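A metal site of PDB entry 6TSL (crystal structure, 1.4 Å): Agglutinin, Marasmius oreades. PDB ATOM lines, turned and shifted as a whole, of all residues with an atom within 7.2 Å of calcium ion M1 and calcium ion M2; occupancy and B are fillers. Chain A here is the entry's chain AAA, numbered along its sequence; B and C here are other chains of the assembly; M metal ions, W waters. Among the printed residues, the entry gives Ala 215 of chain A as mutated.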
ATOM      1  N   ARG A 209     -24.795  -0.625   4.003  1.00  0.00           N
ATOM      2  CA  ARG A 209     -23.785  -0.039   3.089  1.00  0.00           C
ATOM      3  C   ARG A 209     -22.642   0.543   3.920  1.00  0.00           C
ATOM      4  O   ARG A 209     -22.935   1.286   4.889  1.00  0.00           O
ATOM      5  CB  ARG A 209     -24.424   1.036   2.229  1.00  0.00           C
ATOM      6  CG  ARG A 209     -25.512   0.507   1.301  1.00  0.00           C
ATOM      7  CD  ARG A 209     -26.299   1.626   0.621  1.00  0.00           C
ATOM      8  NE  ARG A 209     -25.429   2.483  -0.154  1.00  0.00           N
ATOM      9  CZ  ARG A 209     -25.768   3.657  -0.659  1.00  0.00           C
ATOM     10  NH1 ARG A 209     -26.992   4.120  -0.524  1.00  0.00           N
ATOM     11  NH2 ARG A 209     -24.860   4.386  -1.293  1.00  0.00           N
ATOM     12  N   GLU A 210     -21.402   0.297   3.507  1.00  0.00           N
ATOM     13  CA  GLU A 210     -20.177   0.667   4.261  1.00  0.00           C
ATOM     14  C   GLU A 210     -20.212   2.169   4.558  1.00  0.00           C
ATOM     15  O   GLU A 210     -20.286   2.959   3.570  1.00  0.00           O
ATOM     16  CB  GLU A 210     -18.944   0.265   3.450  1.00  0.00           C
ATOM     17  CG  GLU A 210     -17.623   0.687   4.051  1.00  0.00           C
ATOM     18  CD  GLU A 210     -16.422   0.434   3.136  1.00  0.00           C
ATOM     19  OE1 GLU A 210     -15.409   1.120   3.291  1.00  0.00           O
ATOM     20  OE2 GLU A 210     -16.529  -0.418   2.240  1.00  0.00           O
ATOM     21  N   GLN A 211     -20.298   2.535   5.859  1.00  0.00           N
ATOM     22  CA  GLN A 211     -20.256   3.929   6.429  1.00  0.00           C
ATOM     23  C   GLN A 211     -21.569   4.694   6.111  1.00  0.00           C
ATOM     24  O   GLN A 211     -22.061   5.399   7.011  1.00  0.00           O
ATOM     25  CB  GLN A 211     -19.010   4.690   5.938  1.00  0.00           C
ATOM     26  CG  GLN A 211     -17.711   4.125   6.521  1.00  0.00           C
ATOM     27  CD  GLN A 211     -16.580   5.140   6.514  1.00  0.00           C
ATOM     28  OE1 GLN A 211     -16.729   6.277   6.983  1.00  0.00           O
ATOM     29  NE2 GLN A 211     -15.450   4.738   5.978  1.00  0.00           N
ATOM     30  N   ILE A 212     -22.050   4.663   4.860  1.00  0.00           N
ATOM     31  CA  ILE A 212     -23.110   5.596   4.392  1.00  0.00           C
ATOM     32  C   ILE A 212     -24.496   5.125   4.938  1.00  0.00           C
ATOM     33  O   ILE A 212     -25.376   5.983   5.139  1.00  0.00           O
ATOM     34  CB  ILE A 212     -23.099   5.727   2.848  1.00  0.00           C
ATOM     35  CG1 ILE A 212     -23.986   6.896   2.371  1.00  0.00           C
ATOM     36  CG2 ILE A 212     -23.486   4.434   2.188  1.00  0.00           C
ATOM     37  CD1 ILE A 212     -23.505   8.259   2.796  1.00  0.00           C
ATOM     38  N   TYR A 213     -24.667   3.843   5.200  1.00  0.00           N
ATOM     39  CA  TYR A 213     -25.870   3.364   5.959  1.00  0.00           C
ATOM     40  C   TYR A 213     -25.544   2.054   6.641  1.00  0.00           C
ATOM     41  O   TYR A 213     -25.945   0.984   6.149  1.00  0.00           O
ATOM     42  CB  TYR A 213     -27.083   3.233   5.018  1.00  0.00           C
ATOM     43  CG  TYR A 213     -28.383   3.612   5.682  1.00  0.00           C
ATOM     44  CD1 TYR A 213     -28.661   4.943   5.963  1.00  0.00           C
ATOM     45  CD2 TYR A 213     -29.232   2.654   6.204  1.00  0.00           C
ATOM     46  CE1 TYR A 213     -29.811   5.317   6.618  1.00  0.00           C
ATOM     47  CE2 TYR A 213     -30.347   3.000   6.937  1.00  0.00           C
ATOM     48  CZ  TYR A 213     -30.662   4.346   7.112  1.00  0.00           C
ATOM     49  OH  TYR A 213     -31.789   4.711   7.815  1.00  0.00           O
ATOM     50  N   ASP A 214     -24.741   2.135   7.669  1.00  0.00           N
ATOM     51  CA  ASP A 214     -24.257   0.958   8.397  1.00  0.00           C
ATOM     52  C   ASP A 214     -24.942   0.940   9.775  1.00  0.00           C
ATOM     53  O   ASP A 214     -25.993   1.567   9.913  1.00  0.00           O
ATOM     54  CB  ASP A 214     -22.708   0.936   8.435  1.00  0.00           C
ATOM     55  CG  ASP A 214     -22.074   2.067   9.236  1.00  0.00           C
ATOM     56  OD1 ASP A 214     -22.637   3.154   9.268  1.00  0.00           O
ATOM     57  OD2 ASP A 214     -20.907   1.859   9.725  1.00  0.00           O
ATOM     58  N   ALA A 215     -24.415   0.176  10.719  1.00  0.00           N
ATOM     59  CA  ALA A 215     -25.179  -0.152  11.964  1.00  0.00           C
ATOM     60  C   ALA A 215     -25.632   1.149  12.664  1.00  0.00           C
ATOM     61  O   ALA A 215     -26.768   1.180  13.176  1.00  0.00           O
ATOM     62  CB  ALA A 215     -24.336  -1.029  12.883  1.00  0.00           C
ATOM     63  N   ASP A 216     -24.753   2.149  12.755  1.00  0.00           N
ATOM     64  CA  ASP A 216     -25.071   3.382  13.513  1.00  0.00           C
ATOM     65  C   ASP A 216     -26.260   4.116  12.841  1.00  0.00           C
ATOM     66  O   ASP A 216     -27.107   4.650  13.565  1.00  0.00           O
ATOM     67  CB  ASP A 216     -23.840   4.282  13.670  1.00  0.00           C
ATOM     68  CG  ASP A 216     -23.000   4.401  12.424  1.00  0.00           C
ATOM     69  OD1 ASP A 216     -23.302   5.282  11.599  1.00  0.00           O
ATOM     70  OD2 ASP A 216     -22.093   3.524  12.237  1.00  0.00           O
ATOM     71  N   ASP A 217     -26.379   4.020  11.533  1.00  0.00           N
ATOM     72  CA  ASP A 217     -27.512   4.672  10.799  1.00  0.00           C
ATOM     73  C   ASP A 217     -28.827   3.923  11.133  1.00  0.00           C
ATOM     74  O   ASP A 217     -29.850   4.611  11.372  1.00  0.00           O
ATOM     75  CB  ASP A 217     -27.246   4.727   9.320  1.00  0.00           C
ATOM     76  CG  ASP A 217     -26.005   5.554   8.980  1.00  0.00           C
ATOM     77  OD1 ASP A 217     -26.097   6.782   9.096  1.00  0.00           O
ATOM     78  OD2 ASP A 217     -24.957   4.963   8.833  1.00  0.00           O
ATOM     79  N   PHE A 218     -28.796   2.601  11.160  1.00  0.00           N
ATOM     80  CA  PHE A 218     -30.008   1.778  11.485  1.00  0.00           C
ATOM     81  C   PHE A 218     -30.465   2.101  12.917  1.00  0.00           C
ATOM     82  O   PHE A 218     -31.654   2.311  13.135  1.00  0.00           O
ATOM     83  CB  PHE A 218     -29.720   0.298  11.317  1.00  0.00           C
ATOM     84  CG  PHE A 218     -29.781  -0.197   9.905  1.00  0.00           C
ATOM     85  CD1 PHE A 218     -28.662  -0.117   9.072  1.00  0.00           C
ATOM     86  CD2 PHE A 218     -30.921  -0.800   9.411  1.00  0.00           C
ATOM     87  CE1 PHE A 218     -28.696  -0.649   7.788  1.00  0.00           C
ATOM     88  CE2 PHE A 218     -30.964  -1.301   8.123  1.00  0.00           C
ATOM     89  CZ  PHE A 218     -29.856  -1.212   7.317  1.00  0.00           C
ATOM     90  N   ALA A 258     -23.538  -1.088  16.432  1.00  0.00           N
ATOM     91  CA  ALA A 258     -24.584  -0.206  17.002  1.00  0.00           C
ATOM     92  C   ALA A 258     -25.946  -0.900  16.900  1.00  0.00           C
ATOM     93  O   ALA A 258     -26.161  -1.645  15.919  1.00  0.00           O
ATOM     94  CB  ALA A 258     -24.592   1.108  16.281  1.00  0.00           C
ATOM     95  N   ILE B 181     -17.273   8.451  18.128  1.00  0.00           N
ATOM     96  CA  ILE B 181     -17.095   8.478  16.651  1.00  0.00           C
ATOM     97  C   ILE B 181     -17.819   7.267  16.052  1.00  0.00           C
ATOM     98  O   ILE B 181     -17.672   6.188  16.585  1.00  0.00           O
ATOM     99  CB  ILE B 181     -15.606   8.496  16.310  1.00  0.00           C
ATOM    100  CG1 ILE B 181     -14.936   9.781  16.810  1.00  0.00           C
ATOM    101  CG2 ILE B 181     -15.386   8.289  14.810  1.00  0.00           C
ATOM    102  CD1 ILE B 181     -13.396   9.756  16.758  1.00  0.00           C
ATOM    103  N   LEU B 182     -18.505   7.456  14.933  1.00  0.00           N
ATOM    104  CA  LEU B 182     -19.402   6.421  14.374  1.00  0.00           C
ATOM    105  C   LEU B 182     -18.837   5.896  13.038  1.00  0.00           C
ATOM    106  O   LEU B 182     -19.201   4.780  12.648  1.00  0.00           O
ATOM    107  CB  LEU B 182     -20.795   7.012  14.187  1.00  0.00           C
ATOM    108  CG  LEU B 182     -21.495   7.479  15.472  1.00  0.00           C
ATOM    109  CD1 LEU B 182     -22.856   8.111  15.141  1.00  0.00           C
ATOM    110  CD2 LEU B 182     -21.665   6.347  16.452  1.00  0.00           C
ATOM    111  N   ASP B 183     -18.109   6.753  12.293  1.00  0.00           N
ATOM    112  CA  ASP B 183     -17.638   6.425  10.918  1.00  0.00           C
ATOM    113  C   ASP B 183     -16.210   6.967  10.732  1.00  0.00           C
ATOM    114  O   ASP B 183     -15.586   7.327  11.753  1.00  0.00           O
ATOM    115  CB  ASP B 183     -18.604   6.971   9.855  1.00  0.00           C
ATOM    116  CG  ASP B 183     -20.035   6.380   9.927  1.00  0.00           C
ATOM    117  OD1 ASP B 183     -20.180   5.161   9.767  1.00  0.00           O
ATOM    118  OD2 ASP B 183     -20.991   7.188  10.048  1.00  0.00           O
ATOM    119  N   GLY B 184     -15.694   6.904   9.521  1.00  0.00           N
ATOM    120  CA  GLY B 184     -14.247   7.130   9.246  1.00  0.00           C
ATOM    121  C   GLY B 184     -14.018   8.405   8.440  1.00  0.00           C
ATOM    122  O   GLY B 184     -12.946   8.996   8.604  1.00  0.00           O
ATOM    123  N   TYR B 186     -16.050  11.681   6.235  1.00  0.00           N
ATOM    124  CA  TYR B 186     -17.343  12.407   6.195  1.00  0.00           C
ATOM    125  C   TYR B 186     -17.314  13.464   5.084  1.00  0.00           C
ATOM    126  O   TYR B 186     -16.510  14.418   5.177  1.00  0.00           O
ATOM    127  CB  TYR B 186     -17.630  13.066   7.525  1.00  0.00           C
ATOM    128  CG  TYR B 186     -17.706  12.131   8.688  1.00  0.00           C
ATOM    129  CD1 TYR B 186     -16.566  11.779   9.398  1.00  0.00           C
ATOM    130  CD2 TYR B 186     -18.919  11.642   9.129  1.00  0.00           C
ATOM    131  CE1 TYR B 186     -16.640  11.014  10.553  1.00  0.00           C
ATOM    132  CE2 TYR B 186     -19.006  10.851  10.253  1.00  0.00           C
ATOM    133  CZ  TYR B 186     -17.859  10.521  10.971  1.00  0.00           C
ATOM    134  OH  TYR B 186     -17.945   9.797  12.125  1.00  0.00           O
ATOM    135  N   LYS B 223     -30.207  14.260  12.765  1.00  0.00           N
ATOM    136  CA  LYS B 223     -29.136  13.308  12.408  1.00  0.00           C
ATOM    137  C   LYS B 223     -29.715  12.180  11.523  1.00  0.00           C
ATOM    138  O   LYS B 223     -29.063  11.820  10.548  1.00  0.00           O
ATOM    139  CB  LYS B 223     -28.455  12.720  13.645  1.00  0.00           C
ATOM    140  CG  LYS B 223     -27.286  11.799  13.347  1.00  0.00           C
ATOM    141  CD  LYS B 223     -26.111  11.959  14.300  1.00  0.00           C
ATOM    142  CE  LYS B 223     -24.986  10.955  14.042  1.00  0.00           C
ATOM    143  NZ  LYS B 223     -24.681  10.825  12.588  1.00  0.00           N
ATOM    144  N   PHE B 239     -18.103   6.146   2.814  1.00  0.00           N
ATOM    145  CA  PHE B 239     -18.078   7.463   3.456  1.00  0.00           C
ATOM    146  C   PHE B 239     -19.419   7.700   4.171  1.00  0.00           C
ATOM    147  O   PHE B 239     -20.425   6.993   3.836  1.00  0.00           O
ATOM    148  CB  PHE B 239     -17.815   8.566   2.423  1.00  0.00           C
ATOM    149  CG  PHE B 239     -18.949   8.768   1.459  1.00  0.00           C
ATOM    150  CD1 PHE B 239     -19.220   7.837   0.484  1.00  0.00           C
ATOM    151  CD2 PHE B 239     -19.828   9.828   1.625  1.00  0.00           C
ATOM    152  CE1 PHE B 239     -20.334   7.970  -0.334  1.00  0.00           C
ATOM    153  CE2 PHE B 239     -20.909   9.982   0.776  1.00  0.00           C
ATOM    154  CZ  PHE B 239     -21.169   9.060  -0.182  1.00  0.00           C
ATOM    155  N   ALA B 240     -19.478   8.724   5.000  1.00  0.00           N
ATOM    156  CA  ALA B 240     -20.705   9.181   5.665  1.00  0.00           C
ATOM    157  C   ALA B 240     -20.876  10.683   5.446  1.00  0.00           C
ATOM    158  O   ALA B 240     -19.987  11.301   4.826  1.00  0.00           O
ATOM    159  CB  ALA B 240     -20.646   8.829   7.144  1.00  0.00           C
ATOM    160  N   ILE B 241     -22.022  11.217   5.818  1.00  0.00           N
ATOM    161  CA  ILE B 241     -22.279  12.675   5.798  1.00  0.00           C
ATOM    162  C   ILE B 241     -22.027  13.227   7.189  1.00  0.00           C
ATOM    163  O   ILE B 241     -22.544  12.611   8.187  1.00  0.00           O
ATOM    164  CB  ILE B 241     -23.719  12.976   5.333  1.00  0.00           C
ATOM    165  CG1 ILE B 241     -24.127  12.151   4.102  1.00  0.00           C
ATOM    166  CG2 ILE B 241     -23.892  14.465   5.086  1.00  0.00           C
ATOM    167  CD1 ILE B 241     -23.184  12.284   2.937  1.00  0.00           C
ATOM    168  N   TYR B 293     -21.071  11.452  16.362  1.00  0.00           N
ATOM    169  CA  TYR B 293     -20.957  11.928  14.970  1.00  0.00           C
ATOM    170  C   TYR B 293     -20.266  10.866  14.154  1.00  0.00           C
ATOM    171  O   TYR B 293     -20.520  10.729  12.966  1.00  0.00           O
ATOM    172  CB  TYR B 293     -20.198  13.255  14.911  1.00  0.00           C
ATOM    173  CG  TYR B 293     -18.824  13.219  15.568  1.00  0.00           C
ATOM    174  CD1 TYR B 293     -18.671  13.416  16.932  1.00  0.00           C
ATOM    175  CD2 TYR B 293     -17.685  13.025  14.804  1.00  0.00           C
ATOM    176  CE1 TYR B 293     -17.414  13.411  17.523  1.00  0.00           C
ATOM    177  CE2 TYR B 293     -16.416  13.028  15.383  1.00  0.00           C
ATOM    178  CZ  TYR B 293     -16.276  13.243  16.746  1.00  0.00           C
ATOM    179  OH  TYR B 293     -15.013  13.247  17.318  1.00  0.00           O
ATOM    180  OXT TYR B 293     -19.447  10.106  14.702  1.00  0.00           O
ATOM    181  N   VAL C   2     -14.533   1.172  15.529  1.00  0.00           N
ATOM    182  CA  VAL C   2     -15.626   2.100  15.166  1.00  0.00           C
ATOM    183  C   VAL C   2     -16.842   1.271  14.740  1.00  0.00           C
ATOM    184  O   VAL C   2     -16.703   0.253  14.058  1.00  0.00           O
ATOM    185  CB  VAL C   2     -15.189   3.077  14.050  1.00  0.00           C
ATOM    186  CG1 VAL C   2     -14.890   2.351  12.734  1.00  0.00           C
ATOM    187  CG2 VAL C   2     -16.215   4.177  13.826  1.00  0.00           C
ATOM    188  N   PRO C   3     -18.069   1.641  15.187  1.00  0.00           N
ATOM    189  CA  PRO C   3     -19.251   0.785  14.983  1.00  0.00           C
ATOM    190  C   PRO C   3     -19.578   0.600  13.497  1.00  0.00           C
ATOM    191  O   PRO C   3     -19.577   1.591  12.754  1.00  0.00           O
ATOM    192  CB  PRO C   3     -20.417   1.522  15.726  1.00  0.00           C
ATOM    193  CG  PRO C   3     -19.847   2.919  16.076  1.00  0.00           C
ATOM    194  CD  PRO C   3     -18.344   2.755  16.097  1.00  0.00           C
ATOM    195  N   ARG C   4     -19.844  -0.623  13.117  1.00  0.00           N
ATOM    196  CA  ARG C   4     -20.207  -0.974  11.718  1.00  0.00           C
ATOM    197  C   ARG C   4     -21.349  -1.981  11.752  1.00  0.00           C
ATOM    198  O   ARG C   4     -22.137  -2.067  10.752  1.00  0.00           O
ATOM    199  CB  ARG C   4     -19.000  -1.551  10.968  1.00  0.00           C
ATOM    200  CG  ARG C   4     -17.843  -0.570  10.805  1.00  0.00           C
ATOM    201  CD  ARG C   4     -16.597  -1.231  10.226  1.00  0.00           C
ATOM    202  NE  ARG C   4     -16.823  -1.833   8.905  1.00  0.00           N
ATOM    203  CZ  ARG C   4     -17.019  -3.145   8.678  1.00  0.00           C
ATOM    204  NH1 ARG C   4     -17.022  -4.000   9.686  1.00  0.00           N
ATOM    205  NH2 ARG C   4     -17.210  -3.579   7.444  1.00  0.00           N
ATOM    206  OXT ARG C   4     -21.526  -2.750  12.768  1.00  0.00           O
HETATM  207 CA    CA M   1     -20.015   3.293  11.232  1.00  0.00          CA
HETATM  208 CA    CA M   2     -22.670   5.490   9.285  1.00  0.00          CA
HETATM  209  O   HOH W   1     -23.668   7.633   8.933  1.00  0.00           O
HETATM  210  O   HOH W   2     -17.746   2.810  10.263  1.00  0.00           O
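Of the 24 residues printed, 5 come within 4 Å of calcium ion M1. The nearest printed residue that does not touch calcium ion M1 is Arg 4 of chain C (4.3 Å).
Calcium ion M1 is bound by O of Leu 182 of chain B, at 2.2 Å. OD2 of Asp 214 is bound to calcium ion M1 (2.3 Å). OD2 of Asp 216 binds calcium ion M1 (2.3 Å). The backbone carbonyl oxygen (O) of Pro 3 of chain C is bound to calcium ion M1 (2.3 Å). Calcium ion M1 is bound by the side-chain carboxylate (OD1) of Asp 183 of chain B (2.4 Å). Calcium ion M1 is bound by water W2 (2.5 Å).
The chain-end carboxylate (OXT) of Tyr 293 of chain B lies within hydrogen-bond range of the backbone NH (N) of Leu 182 of chain B (2.8 Å). O of Arg 209 sits at hydrogen-bond distance from N of Asp 214, 3.4 Å away. The side-chain amide oxygen of Gln 211 is in hydrogen-bond range of the backbone NH of Gly 184 of chain B (2.8 Å). The backbone NH of Asp 183 of chain B lies within hydrogen-bond range of the side-chain hydroxyl of Tyr 186 of chain B (3.1 Å).
Five residues have an atom within 4 Å of calcium ion M2: Gln 211, Asp 214, Asp 216, Asp 217 and Asp 183 of chain B.
OD1 of Asp 214 binds calcium ion M2 (2.3 Å). The backbone carbonyl oxygen (O) of Gln 211 binds calcium ion M2 (2.4 Å). Water W1 is bound to calcium ion M2 (2.4 Å). The side-chain carboxylate (OD2) of Asp 217 binds calcium ion M2. Calcium ion M2 is bound by OD1 of Asp 216 (2.4 Å). Calcium ion M2 is bound by OD2 of Asp 183 of chain B (2.5 Å). Calcium ion M2 is bound by OD1 of Asp 183 of chain B (2.6 Å). Calcium ion M2 has seven donor atoms within binding distance.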
